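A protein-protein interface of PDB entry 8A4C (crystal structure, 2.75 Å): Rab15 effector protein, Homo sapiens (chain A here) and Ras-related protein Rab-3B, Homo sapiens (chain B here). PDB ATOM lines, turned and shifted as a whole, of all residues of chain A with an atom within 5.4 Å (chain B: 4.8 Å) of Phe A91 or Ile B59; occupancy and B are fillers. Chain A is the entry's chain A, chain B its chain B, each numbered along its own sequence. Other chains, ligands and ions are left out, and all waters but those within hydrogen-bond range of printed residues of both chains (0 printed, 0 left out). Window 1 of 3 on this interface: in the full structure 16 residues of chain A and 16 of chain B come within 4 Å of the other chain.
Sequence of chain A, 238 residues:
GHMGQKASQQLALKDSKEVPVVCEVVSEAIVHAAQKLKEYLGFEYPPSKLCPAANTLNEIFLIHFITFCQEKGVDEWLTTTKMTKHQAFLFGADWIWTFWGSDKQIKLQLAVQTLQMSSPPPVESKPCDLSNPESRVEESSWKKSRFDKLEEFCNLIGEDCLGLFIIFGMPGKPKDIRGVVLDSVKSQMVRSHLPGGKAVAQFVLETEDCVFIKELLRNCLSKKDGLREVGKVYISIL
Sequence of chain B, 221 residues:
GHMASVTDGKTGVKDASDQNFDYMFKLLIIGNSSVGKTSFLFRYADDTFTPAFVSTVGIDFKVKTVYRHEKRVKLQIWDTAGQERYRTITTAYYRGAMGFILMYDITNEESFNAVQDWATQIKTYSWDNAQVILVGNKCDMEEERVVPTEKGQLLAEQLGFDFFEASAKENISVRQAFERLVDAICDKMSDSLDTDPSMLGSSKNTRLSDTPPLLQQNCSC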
ATOM      1  N   MET A  83       8.736   7.301  -7.381  1.00  0.00           N
ATOM      2  CA  MET A  83       8.598   5.878  -7.118  1.00  0.00           C
ATOM      3  C   MET A  83       7.559   5.260  -8.042  1.00  0.00           C
ATOM      4  O   MET A  83       6.552   5.885  -8.387  1.00  0.00           O
ATOM      5  CB  MET A  83       8.217   5.664  -5.653  1.00  0.00           C
ATOM      6  CG  MET A  83       9.158   6.373  -4.668  1.00  0.00           C
ATOM      7  SD  MET A  83      10.633   5.447  -4.178  1.00  0.00           S
ATOM      8  CE  MET A  83      11.834   5.799  -5.477  1.00  0.00           C
ATOM      9  N   HIS A  86       4.762  -0.220  -7.455  1.00  0.00           N
ATOM     10  CA  HIS A  86       5.328  -1.194  -6.530  1.00  0.00           C
ATOM     11  C   HIS A  86       6.164  -0.515  -5.456  1.00  0.00           C
ATOM     12  O   HIS A  86       6.045  -0.837  -4.269  1.00  0.00           O
ATOM     13  CB  HIS A  86       6.188  -2.198  -7.294  1.00  0.00           C
ATOM     14  CG  HIS A  86       5.433  -3.003  -8.303  1.00  0.00           C
ATOM     15  ND1 HIS A  86       4.082  -3.252  -8.200  1.00  0.00           N
ATOM     16  CD2 HIS A  86       5.845  -3.626  -9.433  1.00  0.00           C
ATOM     17  CE1 HIS A  86       3.692  -3.987  -9.224  1.00  0.00           C
ATOM     18  NE2 HIS A  86       4.743  -4.228  -9.987  1.00  0.00           N
ATOM     19  N   GLN A  87       7.020   0.430  -5.860  1.00  0.00           N
ATOM     20  CA  GLN A  87       7.886   1.117  -4.907  1.00  0.00           C
ATOM     21  C   GLN A  87       7.094   2.004  -3.955  1.00  0.00           C
ATOM     22  O   GLN A  87       7.417   2.083  -2.763  1.00  0.00           O
ATOM     23  CB  GLN A  87       8.930   1.937  -5.649  1.00  0.00           C
ATOM     24  CG  GLN A  87      10.076   1.127  -6.189  1.00  0.00           C
ATOM     25  CD  GLN A  87      11.095   2.005  -6.855  1.00  0.00           C
ATOM     26  OE1 GLN A  87      10.746   3.006  -7.484  1.00  0.00           O
ATOM     27  NE2 GLN A  87      12.368   1.654  -6.708  1.00  0.00           N
ATOM     28  N   ALA A  88       6.061   2.679  -4.465  1.00  0.00           N
ATOM     29  CA  ALA A  88       5.201   3.476  -3.602  1.00  0.00           C
ATOM     30  C   ALA A  88       4.424   2.599  -2.636  1.00  0.00           C
ATOM     31  O   ALA A  88       4.162   3.019  -1.502  1.00  0.00           O
ATOM     32  CB  ALA A  88       4.244   4.330  -4.434  1.00  0.00           C
ATOM     33  N   PHE A  89       4.055   1.386  -3.055  1.00  0.00           N
ATOM     34  CA  PHE A  89       3.397   0.482  -2.120  1.00  0.00           C
ATOM     35  C   PHE A  89       4.365   0.004  -1.045  1.00  0.00           C
ATOM     36  O   PHE A  89       4.032   0.013   0.141  1.00  0.00           O
ATOM     37  CB  PHE A  89       2.777  -0.708  -2.856  1.00  0.00           C
ATOM     38  CG  PHE A  89       2.103  -1.688  -1.936  1.00  0.00           C
ATOM     39  CD1 PHE A  89       0.848  -1.412  -1.417  1.00  0.00           C
ATOM     40  CD2 PHE A  89       2.721  -2.884  -1.588  1.00  0.00           C
ATOM     41  CE1 PHE A  89       0.222  -2.303  -0.563  1.00  0.00           C
ATOM     42  CE2 PHE A  89       2.100  -3.779  -0.735  1.00  0.00           C
ATOM     43  CZ  PHE A  89       0.852  -3.486  -0.219  1.00  0.00           C
ATOM     44  N   LEU A  90       5.570  -0.403  -1.443  1.00  0.00           N
ATOM     45  CA  LEU A  90       6.503  -1.025  -0.507  1.00  0.00           C
ATOM     46  C   LEU A  90       7.084  -0.015   0.476  1.00  0.00           C
ATOM     47  O   LEU A  90       7.196  -0.302   1.673  1.00  0.00           O
ATOM     48  CB  LEU A  90       7.637  -1.705  -1.271  1.00  0.00           C
ATOM     49  CG  LEU A  90       7.313  -2.955  -2.084  1.00  0.00           C
ATOM     50  CD1 LEU A  90       8.516  -3.340  -2.927  1.00  0.00           C
ATOM     51  CD2 LEU A  90       6.890  -4.095  -1.177  1.00  0.00           C
ATOM     52  N   PHE A  91       7.485   1.156  -0.009  1.00  0.00           N
ATOM     53  CA  PHE A  91       8.243   2.076   0.823  1.00  0.00           C
ATOM     54  C   PHE A  91       7.365   3.072   1.560  1.00  0.00           C
ATOM     55  O   PHE A  91       7.862   3.762   2.454  1.00  0.00           O
ATOM     56  CB  PHE A  91       9.264   2.852  -0.017  1.00  0.00           C
ATOM     57  CG  PHE A  91      10.213   1.984  -0.804  1.00  0.00           C
ATOM     58  CD1 PHE A  91      10.624   0.738  -0.326  1.00  0.00           C
ATOM     59  CD2 PHE A  91      10.704   2.425  -2.029  1.00  0.00           C
ATOM     60  CE1 PHE A  91      11.498  -0.048  -1.058  1.00  0.00           C
ATOM     61  CE2 PHE A  91      11.576   1.646  -2.763  1.00  0.00           C
ATOM     62  CZ  PHE A  91      11.974   0.406  -2.279  1.00  0.00           C
ATOM     63  N   GLY A  92       6.087   3.174   1.203  1.00  0.00           N
ATOM     64  CA  GLY A  92       5.237   4.192   1.786  1.00  0.00           C
ATOM     65  C   GLY A  92       5.590   5.605   1.388  1.00  0.00           C
ATOM     66  O   GLY A  92       5.177   6.551   2.060  1.00  0.00           O
ATOM     67  N   ALA A  93       6.340   5.779   0.308  1.00  0.00           N
ATOM     68  CA  ALA A  93       6.800   7.082  -0.139  1.00  0.00           C
ATOM     69  C   ALA A  93       6.363   7.302  -1.577  1.00  0.00           C
ATOM     70  O   ALA A  93       6.334   6.364  -2.380  1.00  0.00           O
ATOM     71  CB  ALA A  93       8.326   7.201  -0.024  1.00  0.00           C
ATOM     72  N   ARG A 146       0.864   3.143   5.463  1.00  0.00           N
ATOM     73  CA  ARG A 146       1.913   3.875   4.753  1.00  0.00           C
ATOM     74  C   ARG A 146       2.870   4.567   5.713  1.00  0.00           C
ATOM     75  O   ARG A 146       4.044   4.773   5.375  1.00  0.00           O
ATOM     76  CB  ARG A 146       1.302   4.905   3.804  1.00  0.00           C
ATOM     77  CG  ARG A 146       0.346   4.334   2.773  1.00  0.00           C
ATOM     78  CD  ARG A 146       0.227   5.277   1.592  1.00  0.00           C
ATOM     79  NE  ARG A 146       1.425   5.272   0.759  1.00  0.00           N
ATOM     80  CZ  ARG A 146       1.735   6.228  -0.107  1.00  0.00           C
ATOM     81  NH1 ARG A 146       1.002   7.323  -0.219  1.00  0.00           N
ATOM     82  NH2 ARG A 146       2.814   6.085  -0.874  1.00  0.00           N
ATOM     83  N   LYS A 149       5.398   1.842   6.902  1.00  0.00           N
ATOM     84  CA  LYS A 149       6.291   1.523   5.794  1.00  0.00           C
ATOM     85  C   LYS A 149       7.285   2.648   5.533  1.00  0.00           C
ATOM     86  O   LYS A 149       8.457   2.379   5.248  1.00  0.00           O
ATOM     87  CB  LYS A 149       5.484   1.222   4.536  1.00  0.00           C
ATOM     88  CG  LYS A 149       4.599   0.006   4.653  1.00  0.00           C
ATOM     89  CD  LYS A 149       4.053  -0.349   3.303  1.00  0.00           C
ATOM     90  CE  LYS A 149       2.557  -0.554   3.320  1.00  0.00           C
ATOM     91  NZ  LYS A 149       2.007  -0.746   1.954  1.00  0.00           N
ATOM     92  N   LEU A 150       6.842   3.909   5.633  1.00  0.00           N
ATOM     93  CA  LEU A 150       7.770   5.028   5.485  1.00  0.00           C
ATOM     94  C   LEU A 150       8.799   5.051   6.611  1.00  0.00           C
ATOM     95  O   LEU A 150       9.989   5.299   6.366  1.00  0.00           O
ATOM     96  CB  LEU A 150       7.009   6.350   5.427  1.00  0.00           C
ATOM     97  CG  LEU A 150       7.882   7.580   5.159  1.00  0.00           C
ATOM     98  CD1 LEU A 150       8.570   7.442   3.814  1.00  0.00           C
ATOM     99  CD2 LEU A 150       7.069   8.861   5.214  1.00  0.00           C
ATOM    100  N   PHE A 153      11.242   2.252   5.958  1.00  0.00           N
ATOM    101  CA  PHE A 153      12.112   2.647   4.856  1.00  0.00           C
ATOM    102  C   PHE A 153      13.212   3.590   5.335  1.00  0.00           C
ATOM    103  O   PHE A 153      14.398   3.372   5.050  1.00  0.00           O
ATOM    104  CB  PHE A 153      11.265   3.291   3.754  1.00  0.00           C
ATOM    105  CG  PHE A 153      12.054   3.746   2.561  1.00  0.00           C
ATOM    106  CD1 PHE A 153      12.516   2.826   1.641  1.00  0.00           C
ATOM    107  CD2 PHE A 153      12.302   5.090   2.341  1.00  0.00           C
ATOM    108  CE1 PHE A 153      13.238   3.220   0.535  1.00  0.00           C
ATOM    109  CE2 PHE A 153      13.020   5.500   1.232  1.00  0.00           C
ATOM    110  CZ  PHE A 153      13.488   4.558   0.326  1.00  0.00           C
ATOM    111  N   LEU B  28      15.936 -12.977  -6.741  1.00  0.00           N
ATOM    112  CA  LEU B  28      16.551 -11.671  -6.572  1.00  0.00           C
ATOM    113  C   LEU B  28      17.734 -11.558  -7.512  1.00  0.00           C
ATOM    114  O   LEU B  28      18.495 -12.511  -7.675  1.00  0.00           O
ATOM    115  CB  LEU B  28      16.986 -11.428  -5.124  1.00  0.00           C
ATOM    116  CG  LEU B  28      15.871 -10.847  -4.258  1.00  0.00           C
ATOM    117  CD1 LEU B  28      15.109 -11.952  -3.556  1.00  0.00           C
ATOM    118  CD2 LEU B  28      16.439  -9.864  -3.247  1.00  0.00           C
ATOM    119  N   THR B  56      18.893   2.157  -9.868  1.00  0.00           N
ATOM    120  CA  THR B  56      17.764   1.767  -9.033  1.00  0.00           C
ATOM    121  C   THR B  56      17.932   2.341  -7.631  1.00  0.00           C
ATOM    122  O   THR B  56      19.017   2.282  -7.050  1.00  0.00           O
ATOM    123  CB  THR B  56      17.638   0.242  -8.974  1.00  0.00           C
ATOM    124  OG1 THR B  56      17.603  -0.293 -10.302  1.00  0.00           O
ATOM    125  CG2 THR B  56      16.360  -0.180  -8.240  1.00  0.00           C
ATOM    126  N   VAL B  57      16.867   2.931  -7.105  1.00  0.00           N
ATOM    127  CA  VAL B  57      16.832   3.413  -5.732  1.00  0.00           C
ATOM    128  C   VAL B  57      16.117   2.358  -4.903  1.00  0.00           C
ATOM    129  O   VAL B  57      14.921   2.110  -5.094  1.00  0.00           O
ATOM    130  CB  VAL B  57      16.129   4.772  -5.624  1.00  0.00           C
ATOM    131  CG1 VAL B  57      16.092   5.214  -4.176  1.00  0.00           C
ATOM    132  CG2 VAL B  57      16.828   5.807  -6.496  1.00  0.00           C
ATOM    133  N   GLY B  58      16.840   1.725  -3.989  1.00  0.00           N
ATOM    134  CA  GLY B  58      16.226   0.745  -3.113  1.00  0.00           C
ATOM    135  C   GLY B  58      16.085  -0.620  -3.750  1.00  0.00           C
ATOM    136  O   GLY B  58      17.064  -1.365  -3.862  1.00  0.00           O
ATOM    137  N   ILE B  59      14.867  -0.955  -4.175  1.00  0.00           N
ATOM    138  CA  ILE B  59      14.569  -2.267  -4.737  1.00  0.00           C
ATOM    139  C   ILE B  59      13.283  -2.122  -5.541  1.00  0.00           C
ATOM    140  O   ILE B  59      12.455  -1.253  -5.254  1.00  0.00           O
ATOM    141  CB  ILE B  59      14.462  -3.327  -3.606  1.00  0.00           C
ATOM    142  CG1 ILE B  59      14.269  -4.747  -4.142  1.00  0.00           C
ATOM    143  CG2 ILE B  59      13.371  -2.955  -2.607  1.00  0.00           C
ATOM    144  CD1 ILE B  59      14.745  -5.811  -3.200  1.00  0.00           C
ATOM    145  N   ASP B  60      13.142  -2.931  -6.591  1.00  0.00           N
ATOM    146  CA  ASP B  60      11.876  -3.033  -7.307  1.00  0.00           C
ATOM    147  C   ASP B  60      11.683  -4.495  -7.697  1.00  0.00           C
ATOM    148  O   ASP B  60      12.557  -5.329  -7.461  1.00  0.00           O
ATOM    149  CB  ASP B  60      11.846  -2.085  -8.514  1.00  0.00           C
ATOM    150  CG  ASP B  60      10.424  -1.749  -8.969  1.00  0.00           C
ATOM    151  OD1 ASP B  60       9.476  -2.464  -8.572  1.00  0.00           O
ATOM    152  OD2 ASP B  60      10.250  -0.766  -9.721  1.00  0.00           O
ATOM    153  N   PHE B  61      10.526  -4.822  -8.277  1.00  0.00           N
ATOM    154  CA  PHE B  61      10.270  -6.190  -8.711  1.00  0.00           C
ATOM    155  C   PHE B  61       9.307  -6.201  -9.893  1.00  0.00           C
ATOM    156  O   PHE B  61       8.536  -5.263 -10.110  1.00  0.00           O
ATOM    157  CB  PHE B  61       9.727  -7.061  -7.560  1.00  0.00           C
ATOM    158  CG  PHE B  61       8.303  -6.754  -7.169  1.00  0.00           C
ATOM    159  CD1 PHE B  61       8.029  -5.713  -6.297  1.00  0.00           C
ATOM    160  CD2 PHE B  61       7.243  -7.528  -7.643  1.00  0.00           C
ATOM    161  CE1 PHE B  61       6.730  -5.433  -5.922  1.00  0.00           C
ATOM    162  CE2 PHE B  61       5.940  -7.244  -7.280  1.00  0.00           C
ATOM    163  CZ  PHE B  61       5.684  -6.193  -6.422  1.00  0.00           C
ATOM    164  N   TRP B  78      13.046  -9.652  -8.106  1.00  0.00           N
ATOM    165  CA  TRP B  78      13.353  -8.417  -7.399  1.00  0.00           C
ATOM    166  C   TRP B  78      14.718  -7.928  -7.867  1.00  0.00           C
ATOM    167  O   TRP B  78      15.740  -8.576  -7.623  1.00  0.00           O
ATOM    168  CB  TRP B  78      13.331  -8.640  -5.888  1.00  0.00           C
ATOM    169  CG  TRP B  78      11.995  -9.044  -5.329  1.00  0.00           C
ATOM    170  CD1 TRP B  78      11.349 -10.237  -5.504  1.00  0.00           C
ATOM    171  CD2 TRP B  78      11.150  -8.253  -4.487  1.00  0.00           C
ATOM    172  NE1 TRP B  78      10.151 -10.231  -4.833  1.00  0.00           N
ATOM    173  CE2 TRP B  78      10.005  -9.024  -4.199  1.00  0.00           C
ATOM    174  CE3 TRP B  78      11.250  -6.966  -3.950  1.00  0.00           C
ATOM    175  CZ2 TRP B  78       8.967  -8.548  -3.401  1.00  0.00           C
ATOM    176  CZ3 TRP B  78      10.220  -6.496  -3.161  1.00  0.00           C
ATOM    177  CH2 TRP B  78       9.093  -7.285  -2.893  1.00  0.00           C
ATOM    178  N   ASP B  79      14.720  -6.794  -8.552  1.00  0.00           N
ATOM    179  CA  ASP B  79      15.929  -6.079  -8.932  1.00  0.00           C
ATOM    180  C   ASP B  79      16.396  -5.281  -7.715  1.00  0.00           C
ATOM    181  O   ASP B  79      15.655  -4.413  -7.225  1.00  0.00           O
ATOM    182  CB  ASP B  79      15.579  -5.151 -10.094  1.00  0.00           C
ATOM    183  CG  ASP B  79      16.729  -4.266 -10.544  1.00  0.00           C
ATOM    184  OD1 ASP B  79      17.903  -4.478 -10.167  1.00  0.00           O
ATOM    185  OD2 ASP B  79      16.424  -3.260 -11.213  1.00  0.00           O
ATOM    186  N   THR B  80      17.608  -5.550  -7.224  1.00  0.00           N
ATOM    187  CA  THR B  80      18.130  -4.781  -6.105  1.00  0.00           C
ATOM    188  C   THR B  80      19.000  -3.636  -6.609  1.00  0.00           C
ATOM    189  O   THR B  80      19.373  -3.577  -7.779  1.00  0.00           O
ATOM    190  CB  THR B  80      18.936  -5.673  -5.164  1.00  0.00           C
ATOM    191  OG1 THR B  80      20.022  -6.259  -5.888  1.00  0.00           O
ATOM    192  CG2 THR B  80      18.065  -6.761  -4.594  1.00  0.00           C
ATOM    193  N   ILE B  89      18.836  -2.236   2.957  1.00  0.00           N
ATOM    194  CA  ILE B  89      17.410  -2.415   2.672  1.00  0.00           C
ATOM    195  C   ILE B  89      17.198  -3.588   1.719  1.00  0.00           C
ATOM    196  O   ILE B  89      16.277  -4.397   1.912  1.00  0.00           O
ATOM    197  CB  ILE B  89      16.757  -1.110   2.155  1.00  0.00           C
ATOM    198  CG1 ILE B  89      15.308  -1.350   1.739  1.00  0.00           C
ATOM    199  CG2 ILE B  89      17.482  -0.508   0.975  1.00  0.00           C
ATOM    200  CD1 ILE B  89      14.444  -0.147   1.869  1.00  0.00           C
ATOM    201  N   THR B  90      18.108  -3.758   0.747  1.00  0.00           N
ATOM    202  CA  THR B  90      18.038  -4.893  -0.168  1.00  0.00           C
ATOM    203  C   THR B  90      18.203  -6.211   0.578  1.00  0.00           C
ATOM    204  O   THR B  90      17.505  -7.188   0.276  1.00  0.00           O
ATOM    205  CB  THR B  90      19.097  -4.762  -1.261  1.00  0.00           C
ATOM    206  OG1 THR B  90      20.393  -4.667  -0.663  1.00  0.00           O
ATOM    207  CG2 THR B  90      18.852  -3.524  -2.093  1.00  0.00           C
ATOM    208  N   TYR B  93      15.166  -7.799   2.013  1.00  0.00           N
ATOM    209  CA  TYR B  93      14.268  -8.516   1.119  1.00  0.00           C
ATOM    210  C   TYR B  93      14.833  -9.857   0.658  1.00  0.00           C
ATOM    211  O   TYR B  93      14.286 -10.461  -0.269  1.00  0.00           O
ATOM    212  CB  TYR B  93      13.924  -7.641  -0.085  1.00  0.00           C
ATOM    213  CG  TYR B  93      12.987  -6.504   0.245  1.00  0.00           C
ATOM    214  CD1 TYR B  93      13.470  -5.307   0.763  1.00  0.00           C
ATOM    215  CD2 TYR B  93      11.617  -6.627   0.051  1.00  0.00           C
ATOM    216  CE1 TYR B  93      12.618  -4.261   1.074  1.00  0.00           C
ATOM    217  CE2 TYR B  93      10.753  -5.585   0.358  1.00  0.00           C
ATOM    218  CZ  TYR B  93      11.262  -4.406   0.870  1.00  0.00           C
ATOM    219  OH  TYR B  93      10.414  -3.371   1.176  1.00  0.00           O
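O of Phe A91 lies close to N of Leu A150 (3.3 Å).
O of Asp B60 sits at hydrogen-bond distance from N of Asp B79 (2.8 Å).
Among the printed residues, merely in contact across the chains: His A86 with Phe B61 (3.2 Å), Phe A91 with Ile B59 (3.4 Å), His A86 with Asp B60 (3.5 Å), Phe A153 with Ile B89 (3.6 Å) and Leu A90 with Trp B78 (3.6 Å).
Of the 13 printed residues of chain B, 6 touch a printed residue of chain A.
Hydrophobic or aromatic side chains of chain B that line the printed part of chain A: Ile B59, Phe B61, Trp B78 and Ile B89.
Along chain B the printed residues that touch a printed residue of chain A span positions 57 to 89.
Of the 13 printed residues of chain A, 5 touch a printed residue of chain B.
Among the printed residues, 7 pairs touch across the chains.
Among the printed residues, no Asp or Glu carboxylate lies within 4 Å of a Lys or Arg side-chain nitrogen of the other chain.
The side-chain amide nitrogen (NE2) of Gln A87 lies within hydrogen-bond range of the backbone carbonyl oxygen (O) of Val B57, 3.1 Å away.
The side-chain amide nitrogen of Gln A87 lies within hydrogen-bond range of the backbone carbonyl oxygen of Ile B59, 3.3 Å away.
Of chain A, only Gln A87 and Phe A91 come within 4 Å of Ile B59.
Of the printed residues of chain B, Leu A90 touches Trp B78.
Printed residues of chain A within 4 Å of Asp B60: His A86.
Printed residues of chain A within 4 Å of Ile B89: Phe A153.
Phe A89 touches none of the printed residues of chain B.
Ala A88 touches none of the printed residues of chain B.
The nearest residue of chain B that does not touch Phe A91 is Val B57 (4.1 Å).
The nearest printed residue of chain A that does not touch Val B57 is Phe A91 (4.1 Å).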
